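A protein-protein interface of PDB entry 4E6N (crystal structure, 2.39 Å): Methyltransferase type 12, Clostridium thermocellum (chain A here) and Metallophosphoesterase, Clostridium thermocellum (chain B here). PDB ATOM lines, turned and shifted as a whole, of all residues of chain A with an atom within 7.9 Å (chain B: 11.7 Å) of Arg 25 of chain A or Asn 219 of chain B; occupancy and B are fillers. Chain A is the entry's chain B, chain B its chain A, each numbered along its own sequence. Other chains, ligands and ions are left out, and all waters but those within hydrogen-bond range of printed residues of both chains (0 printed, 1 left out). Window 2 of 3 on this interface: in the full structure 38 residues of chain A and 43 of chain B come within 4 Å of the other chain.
The side-chain amide nitrogen of Gln 27 of chain A is in hydrogen-bond range of the backbone carbonyl oxygen of Gly 217 of chain B, at 3.4 Å.
OD1 of Asn 219 of chain B is in hydrogen-bond range of NH1 of Arg 25 of chain A.
The backbone carbonyl oxygen (O) of Pro 26 of chain A lies within hydrogen-bond range of the backbone NH (N) of Ala 220 of chain B (2.8 Å).
The backbone carbonyl oxygen (O) of Lys 218 of chain B lies within hydrogen-bond range of the backbone NH (N) of Thr 28 of chain A, at 2.8 Å.
The backbone NH (N) of Ile 38 of chain A lies within hydrogen-bond range of the backbone carbonyl oxygen (O) of Gln 27 of chain A, 2.9 Å away.
The backbone carbonyl oxygen (O) of Lys 21 of chain A sits at hydrogen-bond distance from the side-chain hydroxyl (OH) of Tyr 40 of chain A (3.3 Å).
Among the printed residues, merely in contact across the chains: Gln 27 of chain A with Lys 218 of chain B (3.2 Å), Thr 28 of chain A with Ala 220 of chain B (3.3 Å), Pro 26 of chain A with Asn 219 of chain B (3.6 Å), Phe 39 of chain A with Leu 198 of chain B (3.6 Å), Phe 39 of chain A with Ala 201 of chain B (3.7 Å), Phe 29 of chain A with Gly 217 of chain B (3.7 Å), Tyr 40 of chain A with Ala 201 of chain B (3.8 Å), Gln 27 of chain A with Asn 219 of chain B (3.8 Å) and Phe 39 of chain A with Ile 222 of chain B (3.9 Å).
Printed residues of chain B within 4 Å of Arg 25 of chain A: Asn 219 (2.5 Å).
Asn 219 of chain B touches three residues of chain A.
No residue of chain B comes within 4 Å of Pro 23 of chain A.
Ser 24 of chain A touches none of the printed residues of chain B.
Pro 26 of chain A touches just these residues of chain B: Asn 219 and Ala 220.
Of chain B, only Lys 218 (2.8 Å) and Ala 220 (3.3 Å) come within 4 Å of Thr 28 of chain A.
Of chain A, only Pro 26 and Thr 28 come within 4 Å of Ala 220 of chain B.
Printed residues of chain A within 4 Å of Leu 198 of chain B: Phe 39 (3.6 Å).
Of the printed residues of chain A, Lys 218 of chain B touches Gln 27 (3.2 Å) and Thr 28 (2.8 Å).
Printed residues of chain A within 4 Å of Ile 222 of chain B: Phe 39.
Of the printed residues of chain B, Phe 29 of chain A touches Gly 217.
Of the printed residues of chain A, Gly 217 of chain B touches Gln 27 (3.4 Å) and Phe 29 (3.7 Å).
Glu 224 of chain B touches none of the printed residues of chain A.
Asn 223 of chain B touches none of the printed residues of chain A.
The nearest residue of chain A that does not touch Asn 219 of chain B is Thr 28 of chain A (4.9 Å).
Of the 12 printed residues of chain A, 7 touch a printed residue of chain B.
Among the printed residues, 13 pairs touch across the chains.
Among the printed residues, no Asp or Glu carboxylate lies within 4 Å of a Lys or Arg side-chain nitrogen of the other chain.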
ATOM      1  N   LYS A  21     -25.277   4.336 -23.670  1.00  0.00           N
ATOM      2  CA  LYS A  21     -23.972   3.715 -23.498  1.00  0.00           C
ATOM      3  C   LYS A  21     -24.139   2.214 -23.417  1.00  0.00           C
ATOM      4  O   LYS A  21     -24.913   1.715 -22.597  1.00  0.00           O
ATOM      5  CB  LYS A  21     -23.291   4.231 -22.225  1.00  0.00           C
ATOM      6  CG  LYS A  21     -23.046   5.727 -22.215  1.00  0.00           C
ATOM      7  CD  LYS A  21     -21.902   6.123 -23.128  1.00  0.00           C
ATOM      8  CE  LYS A  21     -21.800   7.631 -23.236  1.00  0.00           C
ATOM      9  NZ  LYS A  21     -23.152   8.266 -23.328  1.00  0.00           N
ATOM     10  N   ASN A  22     -23.413   1.499 -24.269  1.00  0.00           N
ATOM     11  CA  ASN A  22     -23.437   0.043 -24.281  1.00  0.00           C
ATOM     12  C   ASN A  22     -22.699  -0.484 -23.049  1.00  0.00           C
ATOM     13  O   ASN A  22     -21.528  -0.173 -22.846  1.00  0.00           O
ATOM     14  CB  ASN A  22     -22.795  -0.475 -25.578  1.00  0.00           C
ATOM     15  CG  ASN A  22     -22.898  -1.996 -25.744  1.00  0.00           C
ATOM     16  OD1 ASN A  22     -23.009  -2.746 -24.776  1.00  0.00           O
ATOM     17  ND2 ASN A  22     -22.840  -2.448 -26.992  1.00  0.00           N
ATOM     18  N   PRO A  23     -23.389  -1.290 -22.226  1.00  0.00           N
ATOM     19  CA  PRO A  23     -22.784  -1.850 -21.011  1.00  0.00           C
ATOM     20  C   PRO A  23     -21.550  -2.705 -21.278  1.00  0.00           C
ATOM     21  O   PRO A  23     -20.746  -2.917 -20.371  1.00  0.00           O
ATOM     22  CB  PRO A  23     -23.912  -2.692 -20.411  1.00  0.00           C
ATOM     23  CG  PRO A  23     -25.173  -2.029 -20.907  1.00  0.00           C
ATOM     24  CD  PRO A  23     -24.833  -1.580 -22.308  1.00  0.00           C
ATOM     25  N   SER A  24     -21.377  -3.182 -22.501  1.00  0.00           N
ATOM     26  CA  SER A  24     -20.234  -4.038 -22.773  1.00  0.00           C
ATOM     27  C   SER A  24     -19.019  -3.234 -23.241  1.00  0.00           C
ATOM     28  O   SER A  24     -17.933  -3.793 -23.426  1.00  0.00           O
ATOM     29  CB  SER A  24     -20.597  -5.107 -23.802  1.00  0.00           C
ATOM     30  OG  SER A  24     -20.933  -4.525 -25.053  1.00  0.00           O
ATOM     31  N   ARG A  25     -19.199  -1.925 -23.433  1.00  0.00           N
ATOM     32  CA  ARG A  25     -18.120  -1.080 -23.955  1.00  0.00           C
ATOM     33  C   ARG A  25     -17.775   0.136 -23.089  1.00  0.00           C
ATOM     34  O   ARG A  25     -18.338   1.216 -23.268  1.00  0.00           O
ATOM     35  CB  ARG A  25     -18.400  -0.656 -25.402  1.00  0.00           C
ATOM     36  CG  ARG A  25     -18.284  -1.816 -26.401  1.00  0.00           C
ATOM     37  CD  ARG A  25     -17.426  -1.465 -27.607  1.00  0.00           C
ATOM     38  NE  ARG A  25     -18.174  -0.728 -28.616  1.00  0.00           N
ATOM     39  CZ  ARG A  25     -17.621  -0.121 -29.660  1.00  0.00           C
ATOM     40  NH1 ARG A  25     -16.305  -0.157 -29.831  1.00  0.00           N
ATOM     41  NH2 ARG A  25     -18.386   0.532 -30.525  1.00  0.00           N
ATOM     42  N   PRO A  26     -16.826  -0.045 -22.158  1.00  0.00           N
ATOM     43  CA  PRO A  26     -16.245   1.013 -21.319  1.00  0.00           C
ATOM     44  C   PRO A  26     -15.664   2.139 -22.162  1.00  0.00           C
ATOM     45  O   PRO A  26     -15.021   1.865 -23.172  1.00  0.00           O
ATOM     46  CB  PRO A  26     -15.098   0.295 -20.606  1.00  0.00           C
ATOM     47  CG  PRO A  26     -15.453  -1.142 -20.643  1.00  0.00           C
ATOM     48  CD  PRO A  26     -16.202  -1.356 -21.904  1.00  0.00           C
ATOM     49  N   GLN A  27     -15.863   3.381 -21.737  1.00  0.00           N
ATOM     50  CA  GLN A  27     -15.373   4.529 -22.488  1.00  0.00           C
ATOM     51  C   GLN A  27     -14.681   5.599 -21.650  1.00  0.00           C
ATOM     52  O   GLN A  27     -14.976   5.781 -20.473  1.00  0.00           O
ATOM     53  CB  GLN A  27     -16.506   5.177 -23.285  1.00  0.00           C
ATOM     54  CG  GLN A  27     -16.922   4.404 -24.521  1.00  0.00           C
ATOM     55  CD  GLN A  27     -18.057   5.083 -25.240  1.00  0.00           C
ATOM     56  OE1 GLN A  27     -19.221   4.805 -24.971  1.00  0.00           O
ATOM     57  NE2 GLN A  27     -17.727   5.990 -26.154  1.00  0.00           N
ATOM     58  N   THR A  28     -13.777   6.318 -22.301  1.00  0.00           N
ATOM     59  CA  THR A  28     -13.066   7.425 -21.701  1.00  0.00           C
ATOM     60  C   THR A  28     -13.330   8.717 -22.480  1.00  0.00           C
ATOM     61  O   THR A  28     -13.209   8.752 -23.695  1.00  0.00           O
ATOM     62  CB  THR A  28     -11.564   7.126 -21.666  1.00  0.00           C
ATOM     63  OG1 THR A  28     -11.335   5.972 -20.847  1.00  0.00           O
ATOM     64  CG2 THR A  28     -10.778   8.316 -21.112  1.00  0.00           C
ATOM     65  N   PHE A  29     -13.702   9.771 -21.768  1.00  0.00           N
ATOM     66  CA  PHE A  29     -13.958  11.070 -22.379  1.00  0.00           C
ATOM     67  C   PHE A  29     -12.970  12.112 -21.863  1.00  0.00           C
ATOM     68  O   PHE A  29     -12.551  12.085 -20.699  1.00  0.00           O
ATOM     69  CB  PHE A  29     -15.397  11.539 -22.106  1.00  0.00           C
ATOM     70  CG  PHE A  29     -16.458  10.688 -22.760  1.00  0.00           C
ATOM     71  CD1 PHE A  29     -16.720   9.405 -22.303  1.00  0.00           C
ATOM     72  CD2 PHE A  29     -17.202  11.183 -23.821  1.00  0.00           C
ATOM     73  CE1 PHE A  29     -17.688   8.633 -22.899  1.00  0.00           C
ATOM     74  CE2 PHE A  29     -18.170  10.410 -24.425  1.00  0.00           C
ATOM     75  CZ  PHE A  29     -18.418   9.133 -23.962  1.00  0.00           C
ATOM     76  N   ILE A  38     -16.534   5.945 -18.039  1.00  0.00           N
ATOM     77  CA  ILE A  38     -17.845   5.388 -17.793  1.00  0.00           C
ATOM     78  C   ILE A  38     -17.832   3.901 -18.100  1.00  0.00           C
ATOM     79  O   ILE A  38     -17.267   3.472 -19.101  1.00  0.00           O
ATOM     80  CB  ILE A  38     -18.947   6.130 -18.591  1.00  0.00           C
ATOM     81  CG1 ILE A  38     -20.213   5.284 -18.652  1.00  0.00           C
ATOM     82  CG2 ILE A  38     -18.482   6.433 -19.996  1.00  0.00           C
ATOM     83  CD1 ILE A  38     -21.270   5.935 -19.376  1.00  0.00           C
ATOM     84  N   PHE A  39     -18.434   3.113 -17.221  1.00  0.00           N
ATOM     85  CA  PHE A  39     -18.466   1.673 -17.407  1.00  0.00           C
ATOM     86  C   PHE A  39     -19.567   1.103 -16.510  1.00  0.00           C
ATOM     87  O   PHE A  39     -20.109   1.804 -15.656  1.00  0.00           O
ATOM     88  CB  PHE A  39     -17.102   1.071 -17.050  1.00  0.00           C
ATOM     89  CG  PHE A  39     -16.704   1.330 -15.635  1.00  0.00           C
ATOM     90  CD1 PHE A  39     -16.090   2.527 -15.278  1.00  0.00           C
ATOM     91  CD2 PHE A  39     -16.981   0.398 -14.646  1.00  0.00           C
ATOM     92  CE1 PHE A  39     -15.748   2.775 -13.965  1.00  0.00           C
ATOM     93  CE2 PHE A  39     -16.647   0.644 -13.326  1.00  0.00           C
ATOM     94  CZ  PHE A  39     -16.029   1.830 -12.983  1.00  0.00           C
ATOM     95  N   TYR A  40     -19.887  -0.171 -16.697  1.00  0.00           N
ATOM     96  CA  TYR A  40     -20.945  -0.810 -15.920  1.00  0.00           C
ATOM     97  C   TYR A  40     -20.423  -1.914 -15.002  1.00  0.00           C
ATOM     98  O   TYR A  40     -20.111  -3.014 -15.458  1.00  0.00           O
ATOM     99  CB  TYR A  40     -22.012  -1.389 -16.851  1.00  0.00           C
ATOM    100  CG  TYR A  40     -22.886  -0.356 -17.532  1.00  0.00           C
ATOM    101  CD1 TYR A  40     -24.204  -0.174 -17.139  1.00  0.00           C
ATOM    102  CD2 TYR A  40     -22.397   0.430 -18.575  1.00  0.00           C
ATOM    103  CE1 TYR A  40     -25.018   0.756 -17.764  1.00  0.00           C
ATOM    104  CE2 TYR A  40     -23.200   1.368 -19.208  1.00  0.00           C
ATOM    105  CZ  TYR A  40     -24.514   1.528 -18.799  1.00  0.00           C
ATOM    106  OH  TYR A  40     -25.328   2.461 -19.421  1.00  0.00           O
ATOM    107  N   LEU B 198     -14.441  -1.290 -10.278  1.00  0.00           N
ATOM    108  CA  LEU B 198     -13.748  -1.750 -11.471  1.00  0.00           C
ATOM    109  C   LEU B 198     -13.526  -3.258 -11.401  1.00  0.00           C
ATOM    110  O   LEU B 198     -13.661  -3.958 -12.398  1.00  0.00           O
ATOM    111  CB  LEU B 198     -12.413  -1.017 -11.625  1.00  0.00           C
ATOM    112  CG  LEU B 198     -12.550   0.410 -12.153  1.00  0.00           C
ATOM    113  CD1 LEU B 198     -11.297   1.231 -11.824  1.00  0.00           C
ATOM    114  CD2 LEU B 198     -12.800   0.388 -13.657  1.00  0.00           C
ATOM    115  N   ALA B 201     -16.743  -4.761 -12.230  1.00  0.00           N
ATOM    116  CA  ALA B 201     -16.874  -4.641 -13.679  1.00  0.00           C
ATOM    117  C   ALA B 201     -15.966  -5.631 -14.393  1.00  0.00           C
ATOM    118  O   ALA B 201     -16.366  -6.237 -15.377  1.00  0.00           O
ATOM    119  CB  ALA B 201     -16.563  -3.216 -14.150  1.00  0.00           C
ATOM    120  N   SER B 202     -14.746  -5.785 -13.887  1.00  0.00           N
ATOM    121  CA  SER B 202     -13.776  -6.690 -14.493  1.00  0.00           C
ATOM    122  C   SER B 202     -14.278  -8.126 -14.530  1.00  0.00           C
ATOM    123  O   SER B 202     -14.064  -8.840 -15.504  1.00  0.00           O
ATOM    124  CB  SER B 202     -12.455  -6.636 -13.741  1.00  0.00           C
ATOM    125  OG  SER B 202     -11.612  -7.686 -14.166  1.00  0.00           O
ATOM    126  N   ASN B 204     -17.499  -9.121 -14.353  1.00  0.00           N
ATOM    127  CA  ASN B 204     -18.735  -9.222 -15.128  1.00  0.00           C
ATOM    128  C   ASN B 204     -18.576  -8.828 -16.588  1.00  0.00           C
ATOM    129  O   ASN B 204     -19.539  -8.422 -17.237  1.00  0.00           O
ATOM    130  CB  ASN B 204     -19.834  -8.355 -14.505  1.00  0.00           C
ATOM    131  CG  ASN B 204     -20.249  -8.837 -13.141  1.00  0.00           C
ATOM    132  OD1 ASN B 204     -20.152 -10.026 -12.839  1.00  0.00           O
ATOM    133  ND2 ASN B 204     -20.711  -7.915 -12.298  1.00  0.00           N
ATOM    134  N   LYS B 205     -17.359  -8.957 -17.104  1.00  0.00           N
ATOM    135  CA  LYS B 205     -17.037  -8.526 -18.458  1.00  0.00           C
ATOM    136  C   LYS B 205     -17.462  -9.572 -19.490  1.00  0.00           C
ATOM    137  O   LYS B 205     -18.627  -9.618 -19.899  1.00  0.00           O
ATOM    138  CB  LYS B 205     -15.536  -8.246 -18.553  1.00  0.00           C
ATOM    139  CG  LYS B 205     -15.031  -7.787 -19.911  1.00  0.00           C
ATOM    140  CD  LYS B 205     -13.504  -7.671 -19.888  1.00  0.00           C
ATOM    141  CE  LYS B 205     -12.932  -7.293 -21.246  1.00  0.00           C
ATOM    142  NZ  LYS B 205     -11.449  -7.167 -21.191  1.00  0.00           N
ATOM    143  N   GLY B 217     -16.662   9.848 -27.839  1.00  0.00           N
ATOM    144  CA  GLY B 217     -15.594   9.448 -26.935  1.00  0.00           C
ATOM    145  C   GLY B 217     -14.970   8.122 -27.332  1.00  0.00           C
ATOM    146  O   GLY B 217     -15.471   7.455 -28.238  1.00  0.00           O
ATOM    147  N   LYS B 218     -13.894   7.731 -26.648  1.00  0.00           N
ATOM    148  CA  LYS B 218     -13.116   6.545 -27.033  1.00  0.00           C
ATOM    149  C   LYS B 218     -13.234   5.314 -26.122  1.00  0.00           C
ATOM    150  O   LYS B 218     -13.632   5.410 -24.966  1.00  0.00           O
ATOM    151  CB  LYS B 218     -11.642   6.902 -27.194  1.00  0.00           C
ATOM    152  CG  LYS B 218     -11.022   7.555 -25.983  1.00  0.00           C
ATOM    153  CD  LYS B 218      -9.569   7.938 -26.249  1.00  0.00           C
ATOM    154  CE  LYS B 218      -9.429   8.918 -27.422  1.00  0.00           C
ATOM    155  NZ  LYS B 218      -9.274   8.256 -28.761  1.00  0.00           N
ATOM    156  N   ASN B 219     -12.854   4.159 -26.662  1.00  0.00           N
ATOM    157  CA  ASN B 219     -12.998   2.893 -25.962  1.00  0.00           C
ATOM    158  C   ASN B 219     -11.908   2.676 -24.934  1.00  0.00           C
ATOM    159  O   ASN B 219     -10.733   2.954 -25.184  1.00  0.00           O
ATOM    160  CB  ASN B 219     -13.020   1.713 -26.948  1.00  0.00           C
ATOM    161  CG  ASN B 219     -14.314   1.636 -27.753  1.00  0.00           C
ATOM    162  OD1 ASN B 219     -14.331   1.102 -28.860  1.00  0.00           O
ATOM    163  ND2 ASN B 219     -15.401   2.166 -27.197  1.00  0.00           N
ATOM    164  N   ALA B 220     -12.298   2.170 -23.770  1.00  0.00           N
ATOM    165  CA  ALA B 220     -11.343   1.969 -22.703  1.00  0.00           C
ATOM    166  C   ALA B 220     -11.295   0.502 -22.359  1.00  0.00           C
ATOM    167  O   ALA B 220     -12.262  -0.231 -22.585  1.00  0.00           O
ATOM    168  CB  ALA B 220     -11.731   2.790 -21.483  1.00  0.00           C
ATOM    169  N   ASP B 221     -10.169   0.073 -21.804  1.00  0.00           N
ATOM    170  CA  ASP B 221     -10.046  -1.292 -21.317  1.00  0.00           C
ATOM    171  C   ASP B 221     -10.227  -1.352 -19.798  1.00  0.00           C
ATOM    172  O   ASP B 221      -9.561  -0.635 -19.044  1.00  0.00           O
ATOM    173  CB  ASP B 221      -8.716  -1.916 -21.743  1.00  0.00           C
ATOM    174  CG  ASP B 221      -8.563  -3.345 -21.256  1.00  0.00           C
ATOM    175  OD1 ASP B 221      -7.964  -3.548 -20.175  1.00  0.00           O
ATOM    176  OD2 ASP B 221      -9.047  -4.267 -21.949  1.00  0.00           O
ATOM    177  N   ILE B 222     -11.135  -2.220 -19.369  1.00  0.00           N
ATOM    178  CA  ILE B 222     -11.518  -2.321 -17.973  1.00  0.00           C
ATOM    179  C   ILE B 222     -10.349  -2.766 -17.083  1.00  0.00           C
ATOM    180  O   ILE B 222     -10.196  -2.278 -15.965  1.00  0.00           O
ATOM    181  CB  ILE B 222     -12.767  -3.240 -17.807  1.00  0.00           C
ATOM    182  CG1 ILE B 222     -13.534  -2.877 -16.538  1.00  0.00           C
ATOM    183  CG2 ILE B 222     -12.395  -4.724 -17.874  1.00  0.00           C
ATOM    184  CD1 ILE B 222     -14.267  -1.543 -16.638  1.00  0.00           C
ATOM    185  N   ASN B 223      -9.496  -3.655 -17.584  1.00  0.00           N
ATOM    186  CA  ASN B 223      -8.425  -4.173 -16.749  1.00  0.00           C
ATOM    187  C   ASN B 223      -7.281  -3.191 -16.575  1.00  0.00           C
ATOM    188  O   ASN B 223      -6.621  -3.179 -15.540  1.00  0.00           O
ATOM    189  CB  ASN B 223      -7.945  -5.528 -17.263  1.00  0.00           C
ATOM    190  CG  ASN B 223      -9.014  -6.597 -17.129  1.00  0.00           C
ATOM    191  OD1 ASN B 223      -9.454  -7.196 -18.112  1.00  0.00           O
ATOM    192  ND2 ASN B 223      -9.461  -6.820 -15.904  1.00  0.00           N
ATOM    193  N   GLU B 224      -7.062  -2.357 -17.585  1.00  0.00           N
ATOM    194  CA  GLU B 224      -6.047  -1.317 -17.513  1.00  0.00           C
ATOM    195  C   GLU B 224      -6.496  -0.273 -16.503  1.00  0.00           C
ATOM    196  O   GLU B 224      -5.698   0.190 -15.689  1.00  0.00           O
ATOM    197  CB  GLU B 224      -5.831  -0.653 -18.877  1.00  0.00           C
ATOM    198  CG  GLU B 224      -5.327  -1.583 -19.981  1.00  0.00           C
ATOM    199  CD  GLU B 224      -4.988  -0.845 -21.283  1.00  0.00           C
ATOM    200  OE1 GLU B 224      -4.649   0.361 -21.227  1.00  0.00           O
ATOM    201  OE2 GLU B 224      -5.059  -1.475 -22.365  1.00  0.00           O
ATOM    202  N   LEU B 225      -7.779   0.084 -16.567  1.00  0.00           N
ATOM    203  CA  LEU B 225      -8.376   1.031 -15.633  1.00  0.00           C
ATOM    204  C   LEU B 225      -8.217   0.533 -14.210  1.00  0.00           C
ATOM    205  O   LEU B 225      -7.827   1.289 -13.313  1.00  0.00           O
ATOM    206  CB  LEU B 225      -9.859   1.268 -15.960  1.00  0.00           C
ATOM    207  CG  LEU B 225     -10.082   2.090 -17.238  1.00  0.00           C
ATOM    208  CD1 LEU B 225     -11.543   2.168 -17.609  1.00  0.00           C
ATOM    209  CD2 LEU B 225      -9.498   3.497 -17.081  1.00  0.00           C
